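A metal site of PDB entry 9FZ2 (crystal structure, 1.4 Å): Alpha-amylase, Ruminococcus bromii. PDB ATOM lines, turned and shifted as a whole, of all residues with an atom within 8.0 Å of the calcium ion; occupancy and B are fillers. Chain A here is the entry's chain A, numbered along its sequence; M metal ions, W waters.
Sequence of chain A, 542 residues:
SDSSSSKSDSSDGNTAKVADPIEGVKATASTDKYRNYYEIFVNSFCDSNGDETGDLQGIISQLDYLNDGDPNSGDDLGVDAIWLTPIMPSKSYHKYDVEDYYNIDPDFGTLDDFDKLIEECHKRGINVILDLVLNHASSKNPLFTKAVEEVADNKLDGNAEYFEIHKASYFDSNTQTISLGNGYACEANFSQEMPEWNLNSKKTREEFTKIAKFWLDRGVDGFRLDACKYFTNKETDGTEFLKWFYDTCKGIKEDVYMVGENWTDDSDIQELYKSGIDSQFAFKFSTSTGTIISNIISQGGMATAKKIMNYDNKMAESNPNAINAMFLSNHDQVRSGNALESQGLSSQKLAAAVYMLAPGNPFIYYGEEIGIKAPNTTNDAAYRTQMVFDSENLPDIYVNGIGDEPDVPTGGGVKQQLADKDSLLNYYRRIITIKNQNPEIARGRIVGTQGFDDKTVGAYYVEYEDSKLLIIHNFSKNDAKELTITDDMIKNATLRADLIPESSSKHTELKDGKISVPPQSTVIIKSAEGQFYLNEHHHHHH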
ATOM      1  N   LEU A 134     -32.267  -7.428  34.663  1.00  0.00           N
ATOM      2  CA  LEU A 134     -32.665  -8.638  33.951  1.00  0.00           C
ATOM      3  C   LEU A 134     -31.791  -8.884  32.712  1.00  0.00           C
ATOM      4  O   LEU A 134     -31.753 -10.010  32.216  1.00  0.00           O
ATOM      5  CB  LEU A 134     -34.136  -8.533  33.569  1.00  0.00           C
ATOM      6  CG  LEU A 134     -35.136  -8.449  34.722  1.00  0.00           C
ATOM      7  CD1 LEU A 134     -36.548  -8.382  34.166  1.00  0.00           C
ATOM      8  CD2 LEU A 134     -34.883  -9.556  35.698  1.00  0.00           C
ATOM      9  N   ASN A 135     -31.075  -7.879  32.220  1.00  0.00           N
ATOM     10  CA  ASN A 135     -30.279  -8.081  31.027  1.00  0.00           C
ATOM     11  C   ASN A 135     -29.051  -8.908  31.373  1.00  0.00           C
ATOM     12  O   ASN A 135     -28.579  -9.648  30.520  1.00  0.00           O
ATOM     13  CB  ASN A 135     -29.869  -6.771  30.371  1.00  0.00           C
ATOM     14  CG  ASN A 135     -29.013  -6.967  29.141  1.00  0.00           C
ATOM     15  OD1 ASN A 135     -29.462  -7.529  28.131  1.00  0.00           O
ATOM     16  ND2 ASN A 135     -27.786  -6.483  29.211  1.00  0.00           N
ATOM     17  N   HIS A 136     -28.546  -8.748  32.586  1.00  0.00           N
ATOM     18  CA  HIS A 136     -27.262  -9.333  32.929  1.00  0.00           C
ATOM     19  C   HIS A 136     -27.183  -9.630  34.424  1.00  0.00           C
ATOM     20  O   HIS A 136     -27.947  -9.060  35.199  1.00  0.00           O
ATOM     21  CB  HIS A 136     -26.092  -8.436  32.489  1.00  0.00           C
ATOM     22  CG  HIS A 136     -26.186  -7.000  32.873  1.00  0.00           C
ATOM     23  ND1 HIS A 136     -26.859  -6.081  32.086  1.00  0.00           N
ATOM     24  CD2 HIS A 136     -25.690  -6.328  33.950  1.00  0.00           C
ATOM     25  CE1 HIS A 136     -26.696  -4.902  32.637  1.00  0.00           C
ATOM     26  NE2 HIS A 136     -26.046  -5.035  33.784  1.00  0.00           N
ATOM     27  N   GLU A 164     -26.486 -16.208  27.786  1.00  0.00           N
ATOM     28  CA  GLU A 164     -26.443 -15.980  26.349  1.00  0.00           C
ATOM     29  C   GLU A 164     -25.126 -16.558  25.839  1.00  0.00           C
ATOM     30  O   GLU A 164     -24.250 -15.812  25.388  1.00  0.00           O
ATOM     31  CB  GLU A 164     -26.621 -14.487  26.031  1.00  0.00           C
ATOM     32  CG  GLU A 164     -26.890 -14.208  24.554  1.00  0.00           C
ATOM     33  CD  GLU A 164     -28.326 -14.532  24.229  1.00  0.00           C
ATOM     34  OE1 GLU A 164     -29.216 -13.866  24.798  1.00  0.00           O
ATOM     35  OE2 GLU A 164     -28.575 -15.469  23.445  1.00  0.00           O
ATOM     36  N   GLU A 187     -22.440 -13.415  25.758  1.00  0.00           N
ATOM     37  CA  GLU A 187     -22.711 -12.011  25.453  1.00  0.00           C
ATOM     38  C   GLU A 187     -22.489 -11.188  26.731  1.00  0.00           C
ATOM     39  O   GLU A 187     -22.855 -11.600  27.845  1.00  0.00           O
ATOM     40  CB  GLU A 187     -24.120 -11.790  24.930  1.00  0.00           C
ATOM     41  CG  GLU A 187     -24.396 -10.337  24.524  1.00  0.00           C
ATOM     42  CD  GLU A 187     -25.671 -10.163  23.720  1.00  0.00           C
ATOM     43  OE1 GLU A 187     -26.427 -11.150  23.535  1.00  0.00           O
ATOM     44  OE2 GLU A 187     -25.936  -9.019  23.254  1.00  0.00           O
ATOM     45  N   ALA A 188     -21.812 -10.045  26.577  1.00  0.00           N
ATOM     46  CA  ALA A 188     -21.509  -9.185  27.713  1.00  0.00           C
ATOM     47  C   ALA A 188     -21.267  -7.781  27.187  1.00  0.00           C
ATOM     48  O   ALA A 188     -20.116  -7.353  27.087  1.00  0.00           O
ATOM     49  CB  ALA A 188     -20.309  -9.711  28.504  1.00  0.00           C
ATOM     50  N   ASN A 189     -22.342  -7.048  26.865  1.00  0.00           N
ATOM     51  CA  ASN A 189     -22.187  -5.724  26.309  1.00  0.00           C
ATOM     52  C   ASN A 189     -21.514  -4.742  27.257  1.00  0.00           C
ATOM     53  O   ASN A 189     -20.871  -3.791  26.780  1.00  0.00           O
ATOM     54  CB  ASN A 189     -23.504  -5.180  25.768  1.00  0.00           C
ATOM     55  CG  ASN A 189     -23.997  -5.959  24.576  1.00  0.00           C
ATOM     56  OD1 ASN A 189     -23.461  -5.807  23.476  1.00  0.00           O
ATOM     57  ND2 ASN A 189     -24.978  -6.845  24.750  1.00  0.00           N
ATOM     58  N   PHE A 190     -21.702  -4.901  28.572  1.00  0.00           N
ATOM     59  CA  PHE A 190     -21.338  -3.840  29.506  1.00  0.00           C
ATOM     60  C   PHE A 190     -20.003  -4.059  30.190  1.00  0.00           C
ATOM     61  O   PHE A 190     -19.306  -3.064  30.487  1.00  0.00           O
ATOM     62  CB  PHE A 190     -22.388  -3.657  30.585  1.00  0.00           C
ATOM     63  CG  PHE A 190     -23.667  -3.062  30.037  1.00  0.00           C
ATOM     64  CD1 PHE A 190     -23.789  -1.690  29.849  1.00  0.00           C
ATOM     65  CD2 PHE A 190     -24.779  -3.868  29.789  1.00  0.00           C
ATOM     66  CE1 PHE A 190     -24.956  -1.140  29.386  1.00  0.00           C
ATOM     67  CE2 PHE A 190     -25.935  -3.309  29.270  1.00  0.00           C
ATOM     68  CZ  PHE A 190     -26.030  -1.948  29.092  1.00  0.00           C
ATOM     69  N   PRO A 195     -22.155 -10.942  32.554  1.00  0.00           N
ATOM     70  CA  PRO A 195     -22.703 -11.843  31.544  1.00  0.00           C
ATOM     71  C   PRO A 195     -24.217 -11.712  31.421  1.00  0.00           C
ATOM     72  O   PRO A 195     -24.912 -11.549  32.427  1.00  0.00           O
ATOM     73  CB  PRO A 195     -22.335 -13.202  32.044  1.00  0.00           C
ATOM     74  CG  PRO A 195     -22.233 -13.013  33.532  1.00  0.00           C
ATOM     75  CD  PRO A 195     -21.564 -11.668  33.685  1.00  0.00           C
ATOM     76  N   GLU A 196     -24.681 -11.852  30.173  1.00  0.00           N
ATOM     77  CA  GLU A 196     -26.086 -11.615  29.913  1.00  0.00           C
ATOM     78  C   GLU A 196     -26.911 -12.883  29.995  1.00  0.00           C
ATOM     79  O   GLU A 196     -26.472 -13.970  29.653  1.00  0.00           O
ATOM     80  CB  GLU A 196     -26.291 -10.903  28.577  1.00  0.00           C
ATOM     81  CG  GLU A 196     -25.531  -9.581  28.552  1.00  0.00           C
ATOM     82  CD  GLU A 196     -25.938  -8.562  27.525  1.00  0.00           C
ATOM     83  OE1 GLU A 196     -26.894  -8.762  26.751  1.00  0.00           O
ATOM     84  OE2 GLU A 196     -25.265  -7.503  27.561  1.00  0.00           O
ATOM     85  N   TRP A 197     -28.134 -12.683  30.502  1.00  0.00           N
ATOM     86  CA  TRP A 197     -29.142 -13.738  30.548  1.00  0.00           C
ATOM     87  C   TRP A 197     -29.637 -14.047  29.139  1.00  0.00           C
ATOM     88  O   TRP A 197     -29.749 -13.157  28.312  1.00  0.00           O
ATOM     89  CB  TRP A 197     -30.304 -13.281  31.430  1.00  0.00           C
ATOM     90  CG  TRP A 197     -30.015 -13.110  32.904  1.00  0.00           C
ATOM     91  CD1 TRP A 197     -29.725 -11.942  33.555  1.00  0.00           C
ATOM     92  CD2 TRP A 197     -30.091 -14.115  33.919  1.00  0.00           C
ATOM     93  NE1 TRP A 197     -29.570 -12.168  34.892  1.00  0.00           N
ATOM     94  CE2 TRP A 197     -29.786 -13.496  35.160  1.00  0.00           C
ATOM     95  CE3 TRP A 197     -30.390 -15.473  33.915  1.00  0.00           C
ATOM     96  CZ2 TRP A 197     -29.773 -14.193  36.371  1.00  0.00           C
ATOM     97  CZ3 TRP A 197     -30.379 -16.166  35.117  1.00  0.00           C
ATOM     98  CH2 TRP A 197     -30.055 -15.551  36.327  1.00  0.00           C
ATOM     99  N   ASN A 198     -30.051 -15.302  28.918  1.00  0.00           N
ATOM    100  CA  ASN A 198     -30.822 -15.665  27.752  1.00  0.00           C
ATOM    101  C   ASN A 198     -32.293 -15.490  28.070  1.00  0.00           C
ATOM    102  O   ASN A 198     -32.860 -16.275  28.812  1.00  0.00           O
ATOM    103  CB  ASN A 198     -30.439 -17.078  27.314  1.00  0.00           C
ATOM    104  CG  ASN A 198     -31.146 -17.466  26.036  1.00  0.00           C
ATOM    105  OD1 ASN A 198     -32.123 -16.847  25.639  1.00  0.00           O
ATOM    106  ND2 ASN A 198     -30.619 -18.473  25.364  1.00  0.00           N
ATOM    107  N   LEU A 199     -32.884 -14.405  27.535  1.00  0.00           N
ATOM    108  CA  LEU A 199     -34.237 -14.016  27.874  1.00  0.00           C
ATOM    109  C   LEU A 199     -35.275 -14.910  27.211  1.00  0.00           C
ATOM    110  O   LEU A 199     -36.439 -14.786  27.581  1.00  0.00           O
ATOM    111  CB  LEU A 199     -34.400 -12.569  27.470  1.00  0.00           C
ATOM    112  CG  LEU A 199     -33.411 -11.627  28.136  1.00  0.00           C
ATOM    113  CD1 LEU A 199     -33.708 -10.235  27.728  1.00  0.00           C
ATOM    114  CD2 LEU A 199     -33.432 -11.720  29.661  1.00  0.00           C
ATOM    115  N   ALA A 227     -31.292  -1.309  30.918  1.00  0.00           N
ATOM    116  CA  ALA A 227     -30.682  -1.960  29.748  1.00  0.00           C
ATOM    117  C   ALA A 227     -31.714  -2.646  28.867  1.00  0.00           C
ATOM    118  O   ALA A 227     -31.409  -3.655  28.231  1.00  0.00           O
ATOM    119  CB  ALA A 227     -29.591  -2.939  30.204  1.00  0.00           C
ATOM    120  N   CYS A 228     -32.924  -2.078  28.762  1.00  0.00           N
ATOM    121  CA  CYS A 228     -33.953  -2.609  27.869  1.00  0.00           C
ATOM    122  C   CYS A 228     -33.526  -2.614  26.392  1.00  0.00           C
ATOM    123  O   CYS A 228     -33.997  -3.453  25.615  1.00  0.00           O
ATOM    124  CB  CYS A 228     -35.254  -1.815  27.990  1.00  0.00           C
ATOM    125  SG  CYS A 228     -36.094  -1.944  29.591  1.00  0.00           S
ATOM    126  N   LYS A 229     -32.623  -1.704  26.008  1.00  0.00           N
ATOM    127  CA  LYS A 229     -32.067  -1.663  24.647  1.00  0.00           C
ATOM    128  C   LYS A 229     -31.425  -3.019  24.318  1.00  0.00           C
ATOM    129  O   LYS A 229     -31.354  -3.400  23.146  1.00  0.00           O
ATOM    130  CB  LYS A 229     -30.994  -0.572  24.544  1.00  0.00           C
ATOM    131  CG  LYS A 229     -30.066  -0.669  23.323  1.00  0.00           C
ATOM    132  CD  LYS A 229     -29.132   0.516  23.086  1.00  0.00           C
ATOM    133  CE  LYS A 229     -28.784   0.593  21.615  1.00  0.00           C
ATOM    134  NZ  LYS A 229     -27.679   1.512  21.332  1.00  0.00           N
ATOM    135  N   TYR A 230     -30.905  -3.697  25.343  1.00  0.00           N
ATOM    136  CA  TYR A 230     -30.192  -4.942  25.099  1.00  0.00           C
ATOM    137  C   TYR A 230     -31.038  -6.160  25.434  1.00  0.00           C
ATOM    138  O   TYR A 230     -30.520  -7.267  25.409  1.00  0.00           O
ATOM    139  CB  TYR A 230     -28.911  -4.876  25.901  1.00  0.00           C
ATOM    140  CG  TYR A 230     -27.904  -3.888  25.355  1.00  0.00           C
ATOM    141  CD1 TYR A 230     -27.083  -4.232  24.301  1.00  0.00           C
ATOM    142  CD2 TYR A 230     -27.788  -2.638  25.910  1.00  0.00           C
ATOM    143  CE1 TYR A 230     -26.120  -3.351  23.827  1.00  0.00           C
ATOM    144  CE2 TYR A 230     -26.827  -1.737  25.459  1.00  0.00           C
ATOM    145  CZ  TYR A 230     -25.999  -2.102  24.415  1.00  0.00           C
ATOM    146  OH  TYR A 230     -25.040  -1.250  23.962  1.00  0.00           O
ATOM    147  N   PHE A 231     -32.350  -6.000  25.596  1.00  0.00           N
ATOM    148  CA  PHE A 231     -33.235  -7.159  25.600  1.00  0.00           C
ATOM    149  C   PHE A 231     -33.345  -7.767  24.196  1.00  0.00           C
ATOM    150  O   PHE A 231     -33.326  -8.969  24.013  1.00  0.00           O
ATOM    151  CB  PHE A 231     -34.607  -6.693  26.102  1.00  0.00           C
ATOM    152  CG  PHE A 231     -34.750  -6.385  27.580  1.00  0.00           C
ATOM    153  CD1 PHE A 231     -33.666  -6.376  28.452  1.00  0.00           C
ATOM    154  CD2 PHE A 231     -35.975  -5.984  28.066  1.00  0.00           C
ATOM    155  CE1 PHE A 231     -33.855  -6.098  29.811  1.00  0.00           C
ATOM    156  CE2 PHE A 231     -36.142  -5.661  29.396  1.00  0.00           C
ATOM    157  CZ  PHE A 231     -35.084  -5.724  30.271  1.00  0.00           C
ATOM    158  N   THR A 232     -33.513  -6.922  23.199  1.00  0.00           N
ATOM    159  CA  THR A 232     -33.571  -7.399  21.826  1.00  0.00           C
ATOM    160  C   THR A 232     -32.169  -7.740  21.346  1.00  0.00           C
ATOM    161  O   THR A 232     -31.239  -6.946  21.533  1.00  0.00           O
ATOM    162  CB  THR A 232     -34.149  -6.289  20.950  1.00  0.00           C
ATOM    163  OG1 THR A 232     -35.513  -6.144  21.351  1.00  0.00           O
ATOM    164  CG2 THR A 232     -34.162  -6.696  19.497  1.00  0.00           C
ATOM    165  N   ASN A 233     -32.060  -8.879  20.649  1.00  0.00           N
ATOM    166  CA  ASN A 233     -30.794  -9.283  20.035  1.00  0.00           C
ATOM    167  C   ASN A 233     -31.113 -10.194  18.854  1.00  0.00           C
ATOM    168  O   ASN A 233     -32.278 -10.338  18.468  1.00  0.00           O
ATOM    169  CB  ASN A 233     -29.820  -9.841  21.045  1.00  0.00           C
ATOM    170  CG  ASN A 233     -30.292 -11.099  21.722  1.00  0.00           C
ATOM    171  OD1 ASN A 233     -31.187 -11.794  21.229  1.00  0.00           O
ATOM    172  ND2 ASN A 233     -29.613 -11.508  22.786  1.00  0.00           N
ATOM    173  N   THR A 236     -33.698 -12.680  20.251  1.00  0.00           N
ATOM    174  CA  THR A 236     -34.630 -12.289  21.290  1.00  0.00           C
ATOM    175  C   THR A 236     -35.415 -11.076  20.805  1.00  0.00           C
ATOM    176  O   THR A 236     -34.858 -10.054  20.423  1.00  0.00           O
ATOM    177  CB  THR A 236     -33.918 -11.956  22.607  1.00  0.00           C
ATOM    178  OG1 THR A 236     -33.058 -13.056  22.888  1.00  0.00           O
ATOM    179  CG2 THR A 236     -34.891 -11.759  23.742  1.00  0.00           C
HETATM  180 CA    CA M   1     -29.253  -9.056  26.298  1.00  0.00          CA
HETATM  181  O   HOH W   1     -29.849 -10.391  28.210  1.00  0.00           O
HETATM  182  O   HOH W   2     -28.276 -11.273  25.717  1.00  0.00           O
HETATM  183  O   HOH W   3     -31.109 -10.223  25.447  1.00  0.00           O
HETATM  184  O   HOH W   4     -28.375  -8.645  24.056  1.00  0.00           O
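The backbone carbonyl oxygen (O) of Asn 135 sits at hydrogen-bond distance from the backbone NH (N) of Trp 197 (3.1 Å).
ND2 of Asn 135 is in hydrogen-bond range of ND1 of His 136 (3.0 Å).
O of Glu 187 sits at hydrogen-bond distance from N of Glu 196.
The backbone carbonyl oxygen (O) of Glu 196 sits at hydrogen-bond distance from the backbone NH (N) of Glu 164, at 2.9 Å.
ND2 of Asn 189 sits at hydrogen-bond distance from OE2 of Glu 196.
Water W2 lies within hydrogen-bond range of OE1 of Glu 187, OE1 of Glu 164 and ND2 of Asn 233.
Water W3 bridges O of Phe 231 (2.9 Å) and ND2 of Asn 233 (3.3 Å).
Water W1 bridges the backbone carbonyl oxygen (O) of Asn 135 and the backbone carbonyl oxygen (O) of Trp 197.
Water W4 bridges OE2 of Glu 187 (2.6 Å) and ND2 of Asn 233 (3.4 Å).
Within 4 Å of the calcium ion: Asn 135, Glu 196 and Tyr 230.
The calcium ion is bound by water W3 (2.4 Å), O of Tyr 230 (2.4 Å), OD1 of Asn 135 (2.4 Å), water W1 (2.4 Å), OE1 of Glu 196 (2.4 Å), water W4 (2.4 Å) and water W2 (2.5 Å).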
